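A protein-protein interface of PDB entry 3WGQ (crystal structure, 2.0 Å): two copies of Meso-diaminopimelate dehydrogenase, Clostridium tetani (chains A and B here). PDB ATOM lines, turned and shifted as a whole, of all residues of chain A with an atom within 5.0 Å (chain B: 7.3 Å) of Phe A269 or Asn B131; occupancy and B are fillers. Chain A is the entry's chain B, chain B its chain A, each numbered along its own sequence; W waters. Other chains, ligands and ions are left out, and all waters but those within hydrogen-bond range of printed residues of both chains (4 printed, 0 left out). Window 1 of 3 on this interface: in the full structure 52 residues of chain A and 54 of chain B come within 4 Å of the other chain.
O of Glu B268 is in hydrogen-bond range of N of Asn A270 (2.8 Å).
The backbone NH of Asn B270 lies within hydrogen-bond range of the backbone carbonyl oxygen of Glu A268, 2.8 Å away.
O of Leu B127 sits close to OD1 of Asn B131 (3.1 Å).
O of Phe B269 lies within hydrogen-bond range of N of Val B253, 2.8 Å away.
ND2 of Asn A270 lies within hydrogen-bond range of OE2 of Glu A268, 3.0 Å away.
The backbone carbonyl oxygen (O) of Met B267 lies within hydrogen-bond range of the backbone NH (N) of Arg B255 (2.9 Å).
N of Leu A271 is in hydrogen-bond range of O of Gly A251 (3.1 Å).
N of Val A253 sits at hydrogen-bond distance from O of Phe A269.
Among the printed residues, pairs that only touch across the chains: Asn A131 with Phe B269 (3.8 Å), Met A267 with Asn B270 (3.6 Å), Glu A268 with Glu B268 (3.9 Å), Glu A268 with Phe B269 (3.1 Å), Phe A269 with Asn B131 (3.8 Å), Phe A269 with Glu B268 (3.2 Å), Asn A270 with Met B267 (3.7 Å), Leu A271 with Val B266 (3.3 Å) and Leu A271 with Met B267 (3.5 Å).
Phe A269 touches two residues of chain B.
Of the printed residues of chain A, Met B267 touches Asn A270 and Leu A271.
Printed residues of chain B within 4 Å of Met A267: Asn B270.
Of the printed residues of chain A, Asn B270 touches Met A267 (3.6 Å) and Glu A268 (2.8 Å).
Printed residues of chain B within 4 Å of Asn A131: Phe B269 (3.8 Å).
Arg B255 touches none of the printed residues of chain A.
Hydrophobic or aromatic side chains of chain A that line the printed part of chain B: Phe A269 and Leu A271.
Along chain B the printed residues that touch a printed residue of chain A span positions 131 to 270.
Among the printed residues, no Asp or Glu carboxylate lies within 4 Å of a Lys or Arg side-chain nitrogen of the other chain.
Asn A131 touches Phe B269, and with the chains exchanged Phe A269 touches Asn B131.
Met A267 touches Asn B270, and with the chains exchanged Asn A270 touches Met B267.
Glu A268 touches its own counterpart, Glu B268.
Glu A268 touches Phe B269, and with the chains exchanged Phe A269 touches Glu B268.
Positions printed for both chains: 127, 128, 131, 253, 267, 268, 269 and 270.
Of the 11 pairs that touch across the chains among the printed residues, 9 have their exchanged pair printed and touching as well.
Water W3 lies within hydrogen-bond range of OE1 of Glu A268 (2.5 Å) and OD1 of Asn B270 (3.1 Å).
Water W1 lies within hydrogen-bond range of OE1 of Glu B268 (2.6 Å) and OD1 of Asn A270 (3.2 Å).
Water W2 lies within hydrogen-bond range of ND2 of Asn A131 (2.7 Å) and ND2 of Asn B131 (2.8 Å).
Water W4 lies within hydrogen-bond range of OE2 of Glu A268 (2.9 Å) and ND2 of Asn B270 (3.2 Å).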
ATOM      1  N   LEU A 127      -2.821 -29.052  28.349  1.00  0.00           N
ATOM      2  CA  LEU A 127      -3.063 -27.941  27.444  1.00  0.00           C
ATOM      3  C   LEU A 127      -4.434 -27.990  26.776  1.00  0.00           C
ATOM      4  O   LEU A 127      -5.072 -26.958  26.607  1.00  0.00           O
ATOM      5  CB  LEU A 127      -1.966 -27.887  26.377  1.00  0.00           C
ATOM      6  CG  LEU A 127      -0.538 -27.871  26.923  1.00  0.00           C
ATOM      7  CD1 LEU A 127       0.423 -27.531  25.787  1.00  0.00           C
ATOM      8  CD2 LEU A 127      -0.409 -26.849  28.052  1.00  0.00           C
ATOM      9  N   PHE A 128      -4.884 -29.172  26.370  1.00  0.00           N
ATOM     10  CA  PHE A 128      -6.201 -29.254  25.746  1.00  0.00           C
ATOM     11  C   PHE A 128      -7.271 -28.925  26.785  1.00  0.00           C
ATOM     12  O   PHE A 128      -8.258 -28.270  26.477  1.00  0.00           O
ATOM     13  CB  PHE A 128      -6.430 -30.649  25.144  1.00  0.00           C
ATOM     14  CG  PHE A 128      -5.793 -30.837  23.786  1.00  0.00           C
ATOM     15  CD1 PHE A 128      -4.869 -29.915  23.301  1.00  0.00           C
ATOM     16  CD2 PHE A 128      -6.126 -31.927  22.993  1.00  0.00           C
ATOM     17  CE1 PHE A 128      -4.285 -30.074  22.038  1.00  0.00           C
ATOM     18  CE2 PHE A 128      -5.547 -32.099  21.727  1.00  0.00           C
ATOM     19  CZ  PHE A 128      -4.629 -31.172  21.247  1.00  0.00           C
ATOM     20  N   ASN A 131      -7.564 -25.254  27.180  1.00  0.00           N
ATOM     21  CA  ASN A 131      -8.241 -24.629  26.064  1.00  0.00           C
ATOM     22  C   ASN A 131      -9.726 -24.936  25.986  1.00  0.00           C
ATOM     23  O   ASN A 131     -10.484 -24.140  25.444  1.00  0.00           O
ATOM     24  CB  ASN A 131      -7.494 -24.929  24.758  1.00  0.00           C
ATOM     25  CG  ASN A 131      -6.276 -24.014  24.584  1.00  0.00           C
ATOM     26  OD1 ASN A 131      -5.160 -24.342  24.994  1.00  0.00           O
ATOM     27  ND2 ASN A 131      -6.508 -22.842  24.020  1.00  0.00           N
ATOM     28  N   GLY A 251      -3.658 -32.929  17.710  1.00  0.00           N
ATOM     29  CA  GLY A 251      -5.059 -32.811  18.038  1.00  0.00           C
ATOM     30  C   GLY A 251      -5.528 -31.384  17.918  1.00  0.00           C
ATOM     31  O   GLY A 251      -4.726 -30.468  17.705  1.00  0.00           O
ATOM     32  N   PHE A 252      -6.832 -31.198  18.083  1.00  0.00           N
ATOM     33  CA  PHE A 252      -7.450 -29.889  17.965  1.00  0.00           C
ATOM     34  C   PHE A 252      -8.530 -29.667  19.019  1.00  0.00           C
ATOM     35  O   PHE A 252      -9.285 -30.585  19.339  1.00  0.00           O
ATOM     36  CB  PHE A 252      -8.134 -29.742  16.600  1.00  0.00           C
ATOM     37  CG  PHE A 252      -7.276 -30.125  15.427  1.00  0.00           C
ATOM     38  CD1 PHE A 252      -7.005 -31.457  15.144  1.00  0.00           C
ATOM     39  CD2 PHE A 252      -6.752 -29.147  14.598  1.00  0.00           C
ATOM     40  CE1 PHE A 252      -6.221 -31.808  14.048  1.00  0.00           C
ATOM     41  CE2 PHE A 252      -5.967 -29.488  13.499  1.00  0.00           C
ATOM     42  CZ  PHE A 252      -5.701 -30.817  13.224  1.00  0.00           C
ATOM     43  N   VAL A 253      -8.591 -28.451  19.554  1.00  0.00           N
ATOM     44  CA  VAL A 253      -9.639 -28.072  20.494  1.00  0.00           C
ATOM     45  C   VAL A 253     -10.274 -26.839  19.873  1.00  0.00           C
ATOM     46  O   VAL A 253      -9.627 -25.801  19.743  1.00  0.00           O
ATOM     47  CB  VAL A 253      -9.107 -27.703  21.884  1.00  0.00           C
ATOM     48  CG1 VAL A 253     -10.235 -27.144  22.721  1.00  0.00           C
ATOM     49  CG2 VAL A 253      -8.524 -28.924  22.562  1.00  0.00           C
ATOM     50  N   MET A 267     -12.741 -20.157  18.142  1.00  0.00           N
ATOM     51  CA  MET A 267     -11.450 -20.197  18.806  1.00  0.00           C
ATOM     52  C   MET A 267     -10.865 -21.579  18.556  1.00  0.00           C
ATOM     53  O   MET A 267     -11.572 -22.590  18.648  1.00  0.00           O
ATOM     54  CB  MET A 267     -11.618 -20.006  20.313  1.00  0.00           C
ATOM     55  CG  MET A 267     -12.329 -18.733  20.721  1.00  0.00           C
ATOM     56  SD  MET A 267     -12.735 -18.752  22.495  1.00  0.00           S
ATOM     57  CE  MET A 267     -11.139 -18.925  23.211  1.00  0.00           C
ATOM     58  N   GLU A 268      -9.578 -21.639  18.250  1.00  0.00           N
ATOM     59  CA  GLU A 268      -8.943 -22.925  18.003  1.00  0.00           C
ATOM     60  C   GLU A 268      -7.551 -23.030  18.601  1.00  0.00           C
ATOM     61  O   GLU A 268      -6.791 -22.061  18.605  1.00  0.00           O
ATOM     62  CB  GLU A 268      -8.859 -23.203  16.488  1.00  0.00           C
ATOM     63  CG  GLU A 268      -8.165 -24.519  16.150  1.00  0.00           C
ATOM     64  CD  GLU A 268      -8.204 -24.877  14.664  1.00  0.00           C
ATOM     65  OE1 GLU A 268      -9.024 -24.302  13.923  1.00  0.00           O
ATOM     66  OE2 GLU A 268      -7.417 -25.757  14.246  1.00  0.00           O
ATOM     67  N   PHE A 269      -7.237 -24.207  19.135  1.00  0.00           N
ATOM     68  CA  PHE A 269      -5.910 -24.494  19.671  1.00  0.00           C
ATOM     69  C   PHE A 269      -5.572 -25.878  19.147  1.00  0.00           C
ATOM     70  O   PHE A 269      -6.384 -26.804  19.254  1.00  0.00           O
ATOM     71  CB  PHE A 269      -5.895 -24.518  21.205  1.00  0.00           C
ATOM     72  CG  PHE A 269      -4.556 -24.905  21.799  1.00  0.00           C
ATOM     73  CD1 PHE A 269      -3.552 -23.952  21.982  1.00  0.00           C
ATOM     74  CD2 PHE A 269      -4.300 -26.223  22.169  1.00  0.00           C
ATOM     75  CE1 PHE A 269      -2.314 -24.310  22.523  1.00  0.00           C
ATOM     76  CE2 PHE A 269      -3.067 -26.597  22.710  1.00  0.00           C
ATOM     77  CZ  PHE A 269      -2.071 -25.632  22.888  1.00  0.00           C
ATOM     78  N   ASN A 270      -4.395 -26.032  18.554  1.00  0.00           N
ATOM     79  CA  ASN A 270      -4.011 -27.344  18.064  1.00  0.00           C
ATOM     80  C   ASN A 270      -2.532 -27.602  18.228  1.00  0.00           C
ATOM     81  O   ASN A 270      -1.750 -26.682  18.453  1.00  0.00           O
ATOM     82  CB  ASN A 270      -4.452 -27.550  16.603  1.00  0.00           C
ATOM     83  CG  ASN A 270      -3.700 -26.678  15.619  1.00  0.00           C
ATOM     84  OD1 ASN A 270      -2.471 -26.713  15.542  1.00  0.00           O
ATOM     85  ND2 ASN A 270      -4.442 -25.908  14.840  1.00  0.00           N
ATOM     86  N   LEU A 271      -2.159 -28.870  18.133  1.00  0.00           N
ATOM     87  CA  LEU A 271      -0.776 -29.282  18.285  1.00  0.00           C
ATOM     88  C   LEU A 271      -0.408 -30.239  17.161  1.00  0.00           C
ATOM     89  O   LEU A 271      -1.228 -31.039  16.719  1.00  0.00           O
ATOM     90  CB  LEU A 271      -0.579 -30.009  19.630  1.00  0.00           C
ATOM     91  CG  LEU A 271      -0.862 -29.255  20.930  1.00  0.00           C
ATOM     92  CD1 LEU A 271      -0.865 -30.239  22.101  1.00  0.00           C
ATOM     93  CD2 LEU A 271       0.191 -28.177  21.149  1.00  0.00           C
ATOM     94  N   GLY B 126      -4.086  -9.944  25.558  1.00  0.00           N
ATOM     95  CA  GLY B 126      -5.073 -10.817  26.160  1.00  0.00           C
ATOM     96  C   GLY B 126      -4.824 -12.263  25.801  1.00  0.00           C
ATOM     97  O   GLY B 126      -3.807 -12.834  26.173  1.00  0.00           O
ATOM     98  N   LEU B 127      -5.755 -12.846  25.056  1.00  0.00           N
ATOM     99  CA  LEU B 127      -5.644 -14.233  24.642  1.00  0.00           C
ATOM    100  C   LEU B 127      -4.355 -14.537  23.883  1.00  0.00           C
ATOM    101  O   LEU B 127      -3.683 -15.528  24.167  1.00  0.00           O
ATOM    102  CB  LEU B 127      -6.865 -14.613  23.801  1.00  0.00           C
ATOM    103  CG  LEU B 127      -8.052 -15.193  24.586  1.00  0.00           C
ATOM    104  CD1 LEU B 127      -8.218 -14.486  25.916  1.00  0.00           C
ATOM    105  CD2 LEU B 127      -9.304 -15.104  23.758  1.00  0.00           C
ATOM    106  N   PHE B 128      -4.001 -13.698  22.915  1.00  0.00           N
ATOM    107  CA  PHE B 128      -2.774 -13.948  22.171  1.00  0.00           C
ATOM    108  C   PHE B 128      -1.554 -13.856  23.083  1.00  0.00           C
ATOM    109  O   PHE B 128      -0.595 -14.597  22.910  1.00  0.00           O
ATOM    110  CB  PHE B 128      -2.649 -12.963  20.997  1.00  0.00           C
ATOM    111  CG  PHE B 128      -3.492 -13.334  19.805  1.00  0.00           C
ATOM    112  CD1 PHE B 128      -4.515 -14.275  19.920  1.00  0.00           C
ATOM    113  CD2 PHE B 128      -3.275 -12.728  18.570  1.00  0.00           C
ATOM    114  CE1 PHE B 128      -5.314 -14.605  18.823  1.00  0.00           C
ATOM    115  CE2 PHE B 128      -4.064 -13.047  17.466  1.00  0.00           C
ATOM    116  CZ  PHE B 128      -5.090 -13.990  17.595  1.00  0.00           C
ATOM    117  N   SER B 129      -1.597 -12.947  24.051  1.00  0.00           N
ATOM    118  CA  SER B 129      -0.483 -12.763  24.988  1.00  0.00           C
ATOM    119  C   SER B 129      -0.271 -14.053  25.776  1.00  0.00           C
ATOM    120  O   SER B 129       0.860 -14.499  25.977  1.00  0.00           O
ATOM    121  CB  SER B 129      -0.796 -11.627  25.963  1.00  0.00           C
ATOM    122  OG  SER B 129      -1.318 -10.501  25.291  1.00  0.00           O
ATOM    123  N   LEU B 130      -1.376 -14.637  26.238  1.00  0.00           N
ATOM    124  CA  LEU B 130      -1.317 -15.879  26.991  1.00  0.00           C
ATOM    125  C   LEU B 130      -0.687 -16.993  26.156  1.00  0.00           C
ATOM    126  O   LEU B 130       0.133 -17.747  26.654  1.00  0.00           O
ATOM    127  CB  LEU B 130      -2.721 -16.298  27.439  1.00  0.00           C
ATOM    128  CG  LEU B 130      -3.266 -15.538  28.653  1.00  0.00           C
ATOM    129  CD1 LEU B 130      -4.775 -15.745  28.776  1.00  0.00           C
ATOM    130  CD2 LEU B 130      -2.545 -16.013  29.904  1.00  0.00           C
ATOM    131  N   ASN B 131      -1.051 -17.090  24.884  1.00  0.00           N
ATOM    132  CA  ASN B 131      -0.483 -18.147  24.056  1.00  0.00           C
ATOM    133  C   ASN B 131       0.974 -17.925  23.637  1.00  0.00           C
ATOM    134  O   ASN B 131       1.698 -18.888  23.365  1.00  0.00           O
ATOM    135  CB  ASN B 131      -1.390 -18.419  22.859  1.00  0.00           C
ATOM    136  CG  ASN B 131      -2.665 -19.164  23.263  1.00  0.00           C
ATOM    137  OD1 ASN B 131      -3.668 -18.557  23.644  1.00  0.00           O
ATOM    138  ND2 ASN B 131      -2.612 -20.483  23.207  1.00  0.00           N
ATOM    139  N   ARG B 132       1.416 -16.672  23.582  1.00  0.00           N
ATOM    140  CA  ARG B 132       2.820 -16.421  23.263  1.00  0.00           C
ATOM    141  C   ARG B 132       3.616 -16.923  24.467  1.00  0.00           C
ATOM    142  O   ARG B 132       4.646 -17.569  24.319  1.00  0.00           O
ATOM    143  CB  ARG B 132       3.103 -14.930  23.084  1.00  0.00           C
ATOM    144  CG  ARG B 132       2.536 -14.336  21.817  1.00  0.00           C
ATOM    145  CD  ARG B 132       2.887 -12.859  21.728  1.00  0.00           C
ATOM    146  NE  ARG B 132       1.989 -12.216  20.789  1.00  0.00           N
ATOM    147  CZ  ARG B 132       1.070 -11.323  21.123  1.00  0.00           C
ATOM    148  NH1 ARG B 132       0.924 -10.944  22.379  1.00  0.00           N
ATOM    149  NH2 ARG B 132       0.284 -10.831  20.184  1.00  0.00           N
ATOM    150  N   LEU B 133       3.122 -16.619  25.662  1.00  0.00           N
ATOM    151  CA  LEU B 133       3.783 -17.052  26.892  1.00  0.00           C
ATOM    152  C   LEU B 133       3.783 -18.574  26.975  1.00  0.00           C
ATOM    153  O   LEU B 133       4.809 -19.190  27.234  1.00  0.00           O
ATOM    154  CB  LEU B 133       3.074 -16.470  28.114  1.00  0.00           C
ATOM    155  CG  LEU B 133       3.565 -16.973  29.479  1.00  0.00           C
ATOM    156  CD1 LEU B 133       5.084 -16.790  29.559  1.00  0.00           C
ATOM    157  CD2 LEU B 133       2.872 -16.222  30.608  1.00  0.00           C
ATOM    158  N   LEU B 134       2.626 -19.182  26.740  1.00  0.00           N
ATOM    159  CA  LEU B 134       2.521 -20.636  26.793  1.00  0.00           C
ATOM    160  C   LEU B 134       3.486 -21.273  25.800  1.00  0.00           C
ATOM    161  O   LEU B 134       4.263 -22.152  26.161  1.00  0.00           O
ATOM    162  CB  LEU B 134       1.083 -21.074  26.489  1.00  0.00           C
ATOM    163  CG  LEU B 134       0.788 -22.577  26.603  1.00  0.00           C
ATOM    164  CD1 LEU B 134       0.963 -23.036  28.039  1.00  0.00           C
ATOM    165  CD2 LEU B 134      -0.630 -22.845  26.142  1.00  0.00           C
ATOM    166  N   GLY B 135       3.440 -20.827  24.547  1.00  0.00           N
ATOM    167  CA  GLY B 135       4.333 -21.384  23.547  1.00  0.00           C
ATOM    168  C   GLY B 135       5.786 -21.309  23.991  1.00  0.00           C
ATOM    169  O   GLY B 135       6.535 -22.282  23.890  1.00  0.00           O
ATOM    170  N   GLU B 136       6.166 -20.145  24.508  1.00  0.00           N
ATOM    171  CA  GLU B 136       7.528 -19.874  24.972  1.00  0.00           C
ATOM    172  C   GLU B 136       7.979 -20.757  26.130  1.00  0.00           C
ATOM    173  O   GLU B 136       9.149 -21.140  26.211  1.00  0.00           O
ATOM    174  CB  GLU B 136       7.610 -18.424  25.423  1.00  0.00           C
ATOM    175  CG  GLU B 136       8.773 -17.659  24.894  1.00  0.00           C
ATOM    176  CD  GLU B 136       8.698 -16.204  25.298  1.00  0.00           C
ATOM    177  OE1 GLU B 136       8.875 -15.904  26.501  1.00  0.00           O
ATOM    178  OE2 GLU B 136       8.446 -15.365  24.412  1.00  0.00           O
ATOM    179  N   SER B 137       7.054 -21.055  27.038  1.00  0.00           N
ATOM    180  CA  SER B 137       7.368 -21.863  28.207  1.00  0.00           C
ATOM    181  C   SER B 137       7.431 -23.353  27.927  1.00  0.00           C
ATOM    182  O   SER B 137       8.290 -24.053  28.462  1.00  0.00           O
ATOM    183  CB  SER B 137       6.344 -21.603  29.311  1.00  0.00           C
ATOM    184  OG  SER B 137       6.349 -20.239  29.681  1.00  0.00           O
ATOM    185  N   THR B 144       8.277 -17.834  17.946  1.00  0.00           N
ATOM    186  CA  THR B 144       6.873 -17.474  18.042  1.00  0.00           C
ATOM    187  C   THR B 144       6.509 -16.498  16.929  1.00  0.00           C
ATOM    188  O   THR B 144       7.249 -15.557  16.644  1.00  0.00           O
ATOM    189  CB  THR B 144       6.563 -16.800  19.394  1.00  0.00           C
ATOM    190  OG1 THR B 144       6.784 -17.733  20.456  1.00  0.00           O
ATOM    191  CG2 THR B 144       5.113 -16.328  19.435  1.00  0.00           C
ATOM    192  N   VAL B 253      -1.377 -17.356  16.558  1.00  0.00           N
ATOM    193  CA  VAL B 253      -0.176 -17.300  17.378  1.00  0.00           C
ATOM    194  C   VAL B 253       0.426 -18.683  17.212  1.00  0.00           C
ATOM    195  O   VAL B 253      -0.129 -19.679  17.676  1.00  0.00           O
ATOM    196  CB  VAL B 253      -0.460 -17.026  18.869  1.00  0.00           C
ATOM    197  CG1 VAL B 253       0.857 -16.990  19.649  1.00  0.00           C
ATOM    198  CG2 VAL B 253      -1.175 -15.703  19.022  1.00  0.00           C
ATOM    199  N   ILE B 254       1.556 -18.747  16.524  1.00  0.00           N
ATOM    200  CA  ILE B 254       2.210 -20.019  16.284  1.00  0.00           C
ATOM    201  C   ILE B 254       3.578 -20.107  16.940  1.00  0.00           C
ATOM    202  O   ILE B 254       4.373 -19.164  16.885  1.00  0.00           O
ATOM    203  CB  ILE B 254       2.367 -20.281  14.768  1.00  0.00           C
ATOM    204  CG1 ILE B 254       0.996 -20.312  14.098  1.00  0.00           C
ATOM    205  CG2 ILE B 254       3.084 -21.608  14.541  1.00  0.00           C
ATOM    206  CD1 ILE B 254       1.057 -20.319  12.582  1.00  0.00           C
ATOM    207  N   ARG B 255       3.828 -21.242  17.581  1.00  0.00           N
ATOM    208  CA  ARG B 255       5.102 -21.503  18.230  1.00  0.00           C
ATOM    209  C   ARG B 255       5.655 -22.746  17.548  1.00  0.00           C
ATOM    210  O   ARG B 255       5.074 -23.836  17.632  1.00  0.00           O
ATOM    211  CB  ARG B 255       4.922 -21.769  19.730  1.00  0.00           C
ATOM    212  CG  ARG B 255       6.216 -22.074  20.475  1.00  0.00           C
ATOM    213  CD  ARG B 255       7.144 -20.871  20.522  1.00  0.00           C
ATOM    214  NE  ARG B 255       8.346 -21.113  21.325  1.00  0.00           N
ATOM    215  CZ  ARG B 255       9.323 -20.221  21.489  1.00  0.00           C
ATOM    216  NH1 ARG B 255       9.237 -19.035  20.906  1.00  0.00           N
ATOM    217  NH2 ARG B 255      10.384 -20.508  22.240  1.00  0.00           N
ATOM    218  N   VAL B 266       4.903 -28.259  16.895  1.00  0.00           N
ATOM    219  CA  VAL B 266       4.180 -27.029  16.580  1.00  0.00           C
ATOM    220  C   VAL B 266       2.920 -26.799  17.427  1.00  0.00           C
ATOM    221  O   VAL B 266       2.087 -27.694  17.584  1.00  0.00           O
ATOM    222  CB  VAL B 266       3.784 -26.989  15.095  1.00  0.00           C
ATOM    223  CG1 VAL B 266       3.053 -25.684  14.784  1.00  0.00           C
ATOM    224  CG2 VAL B 266       5.035 -27.127  14.224  1.00  0.00           C
ATOM    225  N   MET B 267       2.805 -25.594  17.974  1.00  0.00           N
ATOM    226  CA  MET B 267       1.654 -25.195  18.792  1.00  0.00           C
ATOM    227  C   MET B 267       0.959 -24.017  18.102  1.00  0.00           C
ATOM    228  O   MET B 267       1.620 -23.054  17.699  1.00  0.00           O
ATOM    229  CB  MET B 267       2.106 -24.738  20.186  1.00  0.00           C
ATOM    230  CG  MET B 267       2.791 -25.791  21.047  1.00  0.00           C
ATOM    231  SD  MET B 267       3.596 -25.064  22.532  1.00  0.00           S
ATOM    232  CE  MET B 267       2.155 -24.558  23.490  1.00  0.00           C
ATOM    233  N   GLU B 268      -0.364 -24.081  17.967  1.00  0.00           N
ATOM    234  CA  GLU B 268      -1.093 -22.984  17.344  1.00  0.00           C
ATOM    235  C   GLU B 268      -2.404 -22.649  18.041  1.00  0.00           C
ATOM    236  O   GLU B 268      -3.134 -23.537  18.498  1.00  0.00           O
ATOM    237  CB  GLU B 268      -1.400 -23.280  15.877  1.00  0.00           C
ATOM    238  CG  GLU B 268      -2.046 -22.103  15.169  1.00  0.00           C
ATOM    239  CD  GLU B 268      -2.436 -22.402  13.731  1.00  0.00           C
ATOM    240  OE1 GLU B 268      -1.725 -23.180  13.069  1.00  0.00           O
ATOM    241  OE2 GLU B 268      -3.443 -21.838  13.257  1.00  0.00           O
ATOM    242  N   PHE B 269      -2.671 -21.352  18.130  1.00  0.00           N
ATOM    243  CA  PHE B 269      -3.897 -20.823  18.716  1.00  0.00           C
ATOM    244  C   PHE B 269      -4.363 -19.804  17.695  1.00  0.00           C
ATOM    245  O   PHE B 269      -3.557 -18.995  17.230  1.00  0.00           O
ATOM    246  CB  PHE B 269      -3.619 -20.093  20.040  1.00  0.00           C
ATOM    247  CG  PHE B 269      -4.841 -19.452  20.650  1.00  0.00           C
ATOM    248  CD1 PHE B 269      -5.753 -20.211  21.387  1.00  0.00           C
ATOM    249  CD2 PHE B 269      -5.099 -18.099  20.466  1.00  0.00           C
ATOM    250  CE1 PHE B 269      -6.912 -19.631  21.931  1.00  0.00           C
ATOM    251  CE2 PHE B 269      -6.256 -17.501  21.006  1.00  0.00           C
ATOM    252  CZ  PHE B 269      -7.165 -18.276  21.743  1.00  0.00           C
ATOM    253  N   ASN B 270      -5.634 -19.836  17.327  1.00  0.00           N
ATOM    254  CA  ASN B 270      -6.129 -18.850  16.390  1.00  0.00           C
ATOM    255  C   ASN B 270      -7.584 -18.468  16.636  1.00  0.00           C
ATOM    256  O   ASN B 270      -8.335 -19.196  17.298  1.00  0.00           O
ATOM    257  CB  ASN B 270      -5.909 -19.312  14.935  1.00  0.00           C
ATOM    258  CG  ASN B 270      -6.790 -20.473  14.534  1.00  0.00           C
ATOM    259  OD1 ASN B 270      -8.003 -20.443  14.723  1.00  0.00           O
ATOM    260  ND2 ASN B 270      -6.180 -21.502  13.955  1.00  0.00           N
ATOM    261  N   LEU B 306      -1.871 -12.792  32.418  1.00  0.00           N
ATOM    262  CA  LEU B 306      -0.817 -13.739  32.758  1.00  0.00           C
ATOM    263  C   LEU B 306      -0.835 -14.171  34.224  1.00  0.00           C
ATOM    264  O   LEU B 306      -0.293 -15.221  34.565  1.00  0.00           O
ATOM    265  CB  LEU B 306       0.550 -13.142  32.426  1.00  0.00           C
ATOM    266  CG  LEU B 306       0.677 -12.454  31.058  1.00  0.00           C
ATOM    267  CD1 LEU B 306       2.073 -11.893  30.929  1.00  0.00           C
ATOM    268  CD2 LEU B 306       0.371 -13.435  29.924  1.00  0.00           C
ATOM    269  N   PHE B 310      -6.994 -20.034  34.709  1.00  0.00           N
ATOM    270  CA  PHE B 310      -8.179 -20.165  33.867  1.00  0.00           C
ATOM    271  C   PHE B 310      -9.444 -20.541  34.617  1.00  0.00           C
ATOM    272  O   PHE B 310     -10.539 -20.199  34.187  1.00  0.00           O
ATOM    273  CB  PHE B 310      -7.932 -21.167  32.736  1.00  0.00           C
ATOM    274  CG  PHE B 310      -7.170 -20.595  31.565  1.00  0.00           C
ATOM    275  CD1 PHE B 310      -6.568 -19.339  31.647  1.00  0.00           C
ATOM    276  CD2 PHE B 310      -7.014 -21.334  30.398  1.00  0.00           C
ATOM    277  CE1 PHE B 310      -5.823 -18.831  30.588  1.00  0.00           C
ATOM    278  CE2 PHE B 310      -6.271 -20.836  29.331  1.00  0.00           C
ATOM    279  CZ  PHE B 310      -5.673 -19.580  29.425  1.00  0.00           C
HETATM  280  O   HOH W   1      -0.588 -25.488  13.328  1.00  0.00           O
HETATM  281  O   HOH W   2      -4.614 -21.277  25.062  1.00  0.00           O
HETATM  282  O   HOH W   3     -10.194 -22.132  13.340  1.00  0.00           O
HETATM  283  O   HOH W   4      -6.518 -24.088  12.093  1.00  0.00           O
